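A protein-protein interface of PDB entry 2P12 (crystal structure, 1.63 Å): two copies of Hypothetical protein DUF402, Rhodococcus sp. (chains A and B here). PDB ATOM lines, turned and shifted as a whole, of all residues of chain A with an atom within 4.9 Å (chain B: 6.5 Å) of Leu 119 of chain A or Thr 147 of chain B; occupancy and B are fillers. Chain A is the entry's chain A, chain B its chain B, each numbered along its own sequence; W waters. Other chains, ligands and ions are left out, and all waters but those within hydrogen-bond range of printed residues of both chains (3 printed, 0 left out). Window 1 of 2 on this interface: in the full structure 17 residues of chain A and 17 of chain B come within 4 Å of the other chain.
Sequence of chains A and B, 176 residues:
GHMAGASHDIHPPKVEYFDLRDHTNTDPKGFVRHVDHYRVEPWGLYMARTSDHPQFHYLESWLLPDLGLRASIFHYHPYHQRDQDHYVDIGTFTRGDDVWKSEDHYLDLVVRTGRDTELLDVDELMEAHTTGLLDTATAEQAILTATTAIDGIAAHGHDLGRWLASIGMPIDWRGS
The backbone carbonyl oxygen (O) of Ile 143 of chain B sits close to the side-chain hydroxyl (OG1) of Thr 147 of chain B (3.4 Å). The backbone carbonyl oxygen (O) of Leu 144 of chain B lies within hydrogen-bond range of the side-chain hydroxyl (OG1) of Thr 147 of chain B (3.4 Å). OG1 of Thr 148 of chain B is in hydrogen-bond range of O of Leu 144 of chain B (2.7 Å).
Of the 12 printed residues of chain A, 5 touch a printed residue of chain B. Hydrophobic or aromatic side chains of chain A within 4 Å of the printed part of chain B: Leu 119, Val 122 and Ile 150. Of the 13 printed residues of chain B, 6 touch a printed residue of chain A. Along chain B the printed residues that touch a printed residue of chain A span positions 119 to 151. Among the printed residues, 8 pairs touch across the chains.
CB of Thr 117 of chain A touches OD2 of Asp 151 of chain B (3.99 Å). Leu 119 of chain A touches Thr 147 of chain B (CD2 to CG2, 3.8 Å). Val 122 of chain A touches Ile 143 of chain B (CG1 to CD1, 3.6 Å). Leu 144 of chain B touches Val 122 of chain A. Leu 119 of chain B touches Thr 147 of chain A. Thr 147 of chain A touches Ile 150 of chain B (CB to CD1, 3.9 Å). CD1 of Ile 150 of chain A touches CB of Thr 147 of chain B (3.9 Å). CG2 of Ile 150 of chain A touches OD2 of Asp 151 of chain B (3.7 Å).
Printed residues of chain B within 4 Å of Thr 117 of chain A: Asp 151 (3.99 Å). Of chain A, only Leu 119 and Ile 150 come within 4 Å of Thr 147 of chain B. Printed residues of chain A within 4 Å of Asp 151 of chain B: Thr 117 and Ile 150. The nearest residue of chain A that does not touch Thr 147 of chain B is Thr 147 of chain A (4.1 Å).
Leu 119 of chain A touches Thr 147 of chain B, and with the chains exchanged Thr 147 of chain A touches Leu 119 of chain B. Thr 147 of chain A touches Ile 150 of chain B, and with the chains exchanged Ile 150 of chain A touches Thr 147 of chain B. Of the 8 pairs that touch across the chains among the printed residues, 4 have their exchanged pair printed and touching as well.
Water W1 lies within hydrogen-bond range of the side-chain hydroxyl (OG1) of Thr 117 of chain A (2.7 Å), the side-chain carboxylate (OD2) of Asp 151 of chain B (2.7 Å) and the backbone carbonyl oxygen (O) of Ile 150 of chain A (2.9 Å). Water W3 bridges OD2 of Asp 151 of chain B (2.8 Å) and N of Thr 117 of chain A (2.9 Å). Water W2 lies within hydrogen-bond range of the backbone carbonyl oxygen of Thr 117 of chain A (2.8 Å) and the side-chain carboxylate of Asp 151 of chain B (2.9 Å).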
ATOM      1  N   LEU A 107       4.694  23.963  27.958  1.00  0.00           N
ATOM      2  CA  LEU A 107       3.997  24.228  26.695  1.00  0.00           C
ATOM      3  C   LEU A 107       4.668  23.495  25.532  1.00  0.00           C
ATOM      4  O   LEU A 107       5.908  23.308  25.512  1.00  0.00           O
ATOM      5  CB  LEU A 107       3.983  25.720  26.379  1.00  0.00           C
ATOM      6  CG  LEU A 107       3.417  26.675  27.429  1.00  0.00           C
ATOM      7  CD1 LEU A 107       3.450  28.086  26.830  1.00  0.00           C
ATOM      8  CD2 LEU A 107       1.981  26.261  27.821  1.00  0.00           C
ATOM      9  N   ASP A 108       3.863  23.098  24.524  1.00  0.00           N
ATOM     10  CA  ASP A 108       4.474  22.632  23.299  1.00  0.00           C
ATOM     11  C   ASP A 108       3.562  22.968  22.118  1.00  0.00           C
ATOM     12  O   ASP A 108       2.374  23.209  22.315  1.00  0.00           O
ATOM     13  CB  ASP A 108       4.831  21.135  23.352  1.00  0.00           C
ATOM     14  CG  ASP A 108       3.777  20.330  24.046  1.00  0.00           C
ATOM     15  OD1 ASP A 108       3.885  20.190  25.295  1.00  0.00           O
ATOM     16  OD2 ASP A 108       2.876  19.817  23.360  1.00  0.00           O
ATOM     17  N   LEU A 109       4.146  23.028  20.941  1.00  0.00           N
ATOM     18  CA  LEU A 109       3.417  23.332  19.702  1.00  0.00           C
ATOM     19  C   LEU A 109       3.445  22.101  18.783  1.00  0.00           C
ATOM     20  O   LEU A 109       4.501  21.427  18.662  1.00  0.00           O
ATOM     21  CB  LEU A 109       4.088  24.500  18.974  1.00  0.00           C
ATOM     22  CG  LEU A 109       4.352  25.768  19.771  1.00  0.00           C
ATOM     23  CD1 LEU A 109       5.049  26.739  18.888  1.00  0.00           C
ATOM     24  CD2 LEU A 109       3.009  26.337  20.294  1.00  0.00           C
ATOM     25  N   THR A 117      -1.133  25.459  13.625  1.00  0.00           N
ATOM     26  CA  THR A 117      -0.274  25.225  14.792  1.00  0.00           C
ATOM     27  C   THR A 117      -1.201  25.114  15.995  1.00  0.00           C
ATOM     28  O   THR A 117      -2.137  25.918  16.132  1.00  0.00           O
ATOM     29  CB  THR A 117       0.631  26.442  15.068  1.00  0.00           C
ATOM     30  OG1 THR A 117       1.460  26.665  13.938  1.00  0.00           O
ATOM     31  CG2 THR A 117       1.542  26.198  16.256  1.00  0.00           C
ATOM     32  N   GLU A 118      -0.934  24.148  16.868  1.00  0.00           N
ATOM     33  CA  GLU A 118      -1.787  23.902  18.036  1.00  0.00           C
ATOM     34  C   GLU A 118      -0.926  23.991  19.303  1.00  0.00           C
ATOM     35  O   GLU A 118       0.089  23.287  19.398  1.00  0.00           O
ATOM     36  CB  GLU A 118      -2.420  22.510  17.892  1.00  0.00           C
ATOM     37  CG  GLU A 118      -3.413  22.120  18.978  1.00  0.00           C
ATOM     38  CD  GLU A 118      -3.857  20.645  18.883  1.00  0.00           C
ATOM     39  OE1 GLU A 118      -3.177  19.817  18.222  1.00  0.00           O
ATOM     40  OE2 GLU A 118      -4.881  20.322  19.499  1.00  0.00           O
ATOM     41  N   LEU A 119      -1.308  24.866  20.246  1.00  0.00           N
ATOM     42  CA  LEU A 119      -0.572  25.034  21.529  1.00  0.00           C
ATOM     43  C   LEU A 119      -1.174  24.078  22.556  1.00  0.00           C
ATOM     44  O   LEU A 119      -2.380  24.114  22.807  1.00  0.00           O
ATOM     45  CB  LEU A 119      -0.746  26.472  22.018  1.00  0.00           C
ATOM     46  CG  LEU A 119      -0.184  26.737  23.422  1.00  0.00           C
ATOM     47  CD1 LEU A 119       1.354  26.430  23.510  1.00  0.00           C
ATOM     48  CD2 LEU A 119      -0.446  28.217  23.700  1.00  0.00           C
ATOM     49  N   LEU A 120      -0.334  23.193  23.085  1.00  0.00           N
ATOM     50  CA  LEU A 120      -0.781  22.133  24.022  1.00  0.00           C
ATOM     51  C   LEU A 120      -0.168  22.343  25.396  1.00  0.00           C
ATOM     52  O   LEU A 120       0.833  23.039  25.550  1.00  0.00           O
ATOM     53  CB  LEU A 120      -0.380  20.732  23.530  1.00  0.00           C
ATOM     54  CG  LEU A 120      -0.893  20.396  22.126  1.00  0.00           C
ATOM     55  CD1 LEU A 120      -0.331  19.027  21.765  1.00  0.00           C
ATOM     56  CD2 LEU A 120      -2.381  20.391  22.100  1.00  0.00           C
ATOM     57  N   ASP A 121      -0.788  21.717  26.396  1.00  0.00           N
ATOM     58  CA  ASP A 121      -0.240  21.654  27.754  1.00  0.00           C
ATOM     59  C   ASP A 121      -0.251  22.999  28.525  1.00  0.00           C
ATOM     60  O   ASP A 121       0.517  23.179  29.483  1.00  0.00           O
ATOM     61  CB  ASP A 121       1.131  20.976  27.725  1.00  0.00           C
ATOM     62  CG  ASP A 121       1.040  19.530  27.287  1.00  0.00           C
ATOM     63  OD1 ASP A 121       0.030  18.854  27.674  1.00  0.00           O
ATOM     64  OD2 ASP A 121       1.974  19.070  26.615  1.00  0.00           O
ATOM     65  N   VAL A 122      -1.148  23.922  28.145  1.00  0.00           N
ATOM     66  CA  VAL A 122      -1.311  25.164  28.886  1.00  0.00           C
ATOM     67  C   VAL A 122      -1.776  24.834  30.295  1.00  0.00           C
ATOM     68  O   VAL A 122      -1.340  25.482  31.251  1.00  0.00           O
ATOM     69  CB  VAL A 122      -2.273  26.143  28.173  1.00  0.00           C
ATOM     70  CG1 VAL A 122      -2.483  27.393  28.992  1.00  0.00           C
ATOM     71  CG2 VAL A 122      -1.648  26.494  26.769  1.00  0.00           C
ATOM     72  N   ALA A 146       6.073  31.069  23.332  1.00  0.00           N
ATOM     73  CA  ALA A 146       5.055  30.379  22.490  1.00  0.00           C
ATOM     74  C   ALA A 146       4.385  31.321  21.496  1.00  0.00           C
ATOM     75  O   ALA A 146       4.243  30.985  20.296  1.00  0.00           O
ATOM     76  CB  ALA A 146       4.024  29.757  23.386  1.00  0.00           C
ATOM     77  N   THR A 147       3.965  32.501  21.962  1.00  0.00           N
ATOM     78  CA  THR A 147       3.228  33.420  21.054  1.00  0.00           C
ATOM     79  C   THR A 147       4.125  33.978  19.964  1.00  0.00           C
ATOM     80  O   THR A 147       3.666  34.082  18.807  1.00  0.00           O
ATOM     81  CB  THR A 147       2.465  34.547  21.837  1.00  0.00           C
ATOM     82  OG1 THR A 147       3.401  35.359  22.523  1.00  0.00           O
ATOM     83  CG2 THR A 147       1.545  33.945  22.879  1.00  0.00           C
ATOM     84  N   ILE A 150       4.275  31.141  17.532  1.00  0.00           N
ATOM     85  CA  ILE A 150       2.954  30.975  16.838  1.00  0.00           C
ATOM     86  C   ILE A 150       2.800  32.059  15.761  1.00  0.00           C
ATOM     87  O   ILE A 150       2.392  31.805  14.609  1.00  0.00           O
ATOM     88  CB  ILE A 150       1.797  31.023  17.853  1.00  0.00           C
ATOM     89  CG1 ILE A 150       1.749  29.686  18.592  1.00  0.00           C
ATOM     90  CG2 ILE A 150       0.427  31.251  17.107  1.00  0.00           C
ATOM     91  CD1 ILE A 150       0.916  29.728  19.920  1.00  0.00           C
ATOM     92  N   ILE B  90      -9.326  40.332  25.832  1.00  0.00           N
ATOM     93  CA  ILE B  90      -9.697  38.940  25.825  1.00  0.00           C
ATOM     94  C   ILE B  90     -10.605  38.715  27.048  1.00  0.00           C
ATOM     95  O   ILE B  90     -10.288  39.122  28.172  1.00  0.00           O
ATOM     96  CB  ILE B  90      -8.426  38.063  25.835  1.00  0.00           C
ATOM     97  CG1 ILE B  90      -7.778  38.191  24.433  1.00  0.00           C
ATOM     98  CG2 ILE B  90      -8.755  36.615  26.201  1.00  0.00           C
ATOM     99  CD1 ILE B  90      -6.329  38.130  24.424  1.00  0.00           C
ATOM    100  N   LEU B 119       1.246  40.958  22.782  1.00  0.00           N
ATOM    101  CA  LEU B 119       0.401  40.397  23.822  1.00  0.00           C
ATOM    102  C   LEU B 119       0.833  40.983  25.127  1.00  0.00           C
ATOM    103  O   LEU B 119       2.014  40.867  25.503  1.00  0.00           O
ATOM    104  CB  LEU B 119       0.549  38.846  23.918  1.00  0.00           C
ATOM    105  CG  LEU B 119      -0.211  38.122  25.044  1.00  0.00           C
ATOM    106  CD1 LEU B 119      -1.721  38.317  25.042  1.00  0.00           C
ATOM    107  CD2 LEU B 119       0.179  36.621  25.053  1.00  0.00           C
ATOM    108  N   ALA B 142      -8.565  31.841  28.151  1.00  0.00           N
ATOM    109  CA  ALA B 142      -8.035  33.171  27.815  1.00  0.00           C
ATOM    110  C   ALA B 142      -6.777  33.060  26.921  1.00  0.00           C
ATOM    111  O   ALA B 142      -6.639  33.758  25.871  1.00  0.00           O
ATOM    112  CB  ALA B 142      -7.727  33.943  29.088  1.00  0.00           C
ATOM    113  N   ILE B 143      -5.874  32.144  27.297  1.00  0.00           N
ATOM    114  CA  ILE B 143      -4.623  31.954  26.541  1.00  0.00           C
ATOM    115  C   ILE B 143      -4.921  31.432  25.143  1.00  0.00           C
ATOM    116  O   ILE B 143      -4.384  31.929  24.161  1.00  0.00           O
ATOM    117  CB  ILE B 143      -3.621  31.063  27.289  1.00  0.00           C
ATOM    118  CG1 ILE B 143      -3.057  31.823  28.485  1.00  0.00           C
ATOM    119  CG2 ILE B 143      -2.498  30.651  26.346  1.00  0.00           C
ATOM    120  CD1 ILE B 143      -2.404  30.943  29.599  1.00  0.00           C
ATOM    121  N   LEU B 144      -5.804  30.464  25.057  1.00  0.00           N
ATOM    122  CA  LEU B 144      -6.158  29.883  23.766  1.00  0.00           C
ATOM    123  C   LEU B 144      -6.968  30.855  22.832  1.00  0.00           C
ATOM    124  O   LEU B 144      -6.864  30.791  21.602  1.00  0.00           O
ATOM    125  CB  LEU B 144      -6.786  28.486  23.993  1.00  0.00           C
ATOM    126  CG  LEU B 144      -6.033  27.307  24.692  1.00  0.00           C
ATOM    127  CD1 LEU B 144      -5.114  27.659  25.870  1.00  0.00           C
ATOM    128  CD2 LEU B 144      -7.012  26.282  25.200  1.00  0.00           C
ATOM    129  N   THR B 145      -7.742  31.782  23.407  1.00  0.00           N
ATOM    130  CA  THR B 145      -8.363  32.858  22.670  1.00  0.00           C
ATOM    131  C   THR B 145      -7.291  33.787  22.096  1.00  0.00           C
ATOM    132  O   THR B 145      -7.304  34.142  20.920  1.00  0.00           O
ATOM    133  CB  THR B 145      -9.351  33.660  23.584  1.00  0.00           C
ATOM    134  OG1 THR B 145     -10.529  32.856  23.760  1.00  0.00           O
ATOM    135  CG2 THR B 145      -9.707  34.983  22.923  1.00  0.00           C
ATOM    136  N   ALA B 146      -6.339  34.144  22.939  1.00  0.00           N
ATOM    137  CA  ALA B 146      -5.238  35.028  22.563  1.00  0.00           C
ATOM    138  C   ALA B 146      -4.380  34.418  21.446  1.00  0.00           C
ATOM    139  O   ALA B 146      -4.105  35.083  20.435  1.00  0.00           O
ATOM    140  CB  ALA B 146      -4.390  35.327  23.819  1.00  0.00           C
ATOM    141  N   THR B 147      -4.003  33.141  21.586  1.00  0.00           N
ATOM    142  CA  THR B 147      -3.123  32.523  20.565  1.00  0.00           C
ATOM    143  C   THR B 147      -3.865  32.301  19.248  1.00  0.00           C
ATOM    144  O   THR B 147      -3.273  32.415  18.190  1.00  0.00           O
ATOM    145  CB  THR B 147      -2.482  31.198  21.108  1.00  0.00           C
ATOM    146  OG1 THR B 147      -3.526  30.238  21.347  1.00  0.00           O
ATOM    147  CG2 THR B 147      -1.744  31.533  22.387  1.00  0.00           C
ATOM    148  N   THR B 148      -5.157  32.000  19.327  1.00  0.00           N
ATOM    149  CA  THR B 148      -6.011  31.797  18.139  1.00  0.00           C
ATOM    150  C   THR B 148      -6.047  33.115  17.345  1.00  0.00           C
ATOM    151  O   THR B 148      -5.859  33.149  16.118  1.00  0.00           O
ATOM    152  CB  THR B 148      -7.443  31.373  18.517  1.00  0.00           C
ATOM    153  OG1 THR B 148      -7.404  30.057  19.075  1.00  0.00           O
ATOM    154  CG2 THR B 148      -8.336  31.349  17.265  1.00  0.00           C
ATOM    155  N   ALA B 149      -6.193  34.200  18.087  1.00  0.00           N
ATOM    156  CA  ALA B 149      -6.219  35.519  17.464  1.00  0.00           C
ATOM    157  C   ALA B 149      -4.824  35.889  16.903  1.00  0.00           C
ATOM    158  O   ALA B 149      -4.696  36.385  15.788  1.00  0.00           O
ATOM    159  CB  ALA B 149      -6.737  36.566  18.467  1.00  0.00           C
ATOM    160  N   ILE B 150      -3.750  35.662  17.670  1.00  0.00           N
ATOM    161  CA  ILE B 150      -2.422  36.035  17.193  1.00  0.00           C
ATOM    162  C   ILE B 150      -2.128  35.276  15.915  1.00  0.00           C
ATOM    163  O   ILE B 150      -1.534  35.831  14.977  1.00  0.00           O
ATOM    164  CB  ILE B 150      -1.369  35.751  18.318  1.00  0.00           C
ATOM    165  CG1 ILE B 150      -1.585  36.770  19.458  1.00  0.00           C
ATOM    166  CG2 ILE B 150       0.074  35.733  17.770  1.00  0.00           C
ATOM    167  CD1 ILE B 150      -0.818  36.413  20.732  1.00  0.00           C
ATOM    168  N   ASP B 151      -2.506  33.988  15.902  1.00  0.00           N
ATOM    169  CA  ASP B 151      -2.239  33.143  14.722  1.00  0.00           C
ATOM    170  C   ASP B 151      -3.019  33.703  13.513  1.00  0.00           C
ATOM    171  O   ASP B 151      -2.441  33.954  12.403  1.00  0.00           O
ATOM    172  CB  ASP B 151      -2.668  31.693  15.041  1.00  0.00           C
ATOM    173  CG  ASP B 151      -2.198  30.709  14.017  1.00  0.00           C
ATOM    174  OD1 ASP B 151      -2.438  30.927  12.812  1.00  0.00           O
ATOM    175  OD2 ASP B 151      -1.570  29.701  14.398  1.00  0.00           O
ATOM    176  N   GLY B 152      -4.313  33.922  13.703  1.00  0.00           N
ATOM    177  CA  GLY B 152      -5.152  34.416  12.571  1.00  0.00           C
ATOM    178  C   GLY B 152      -4.679  35.787  12.075  1.00  0.00           C
ATOM    179  O   GLY B 152      -4.568  36.045  10.874  1.00  0.00           O
HETATM  180  O   HOH W   1       1.092  29.345  13.973  1.00  0.00           O
HETATM  181  O   HOH W   2      -2.130  28.608  17.011  1.00  0.00           O
HETATM  182  O   HOH W   3      -3.120  27.571  13.393  1.00  0.00           O
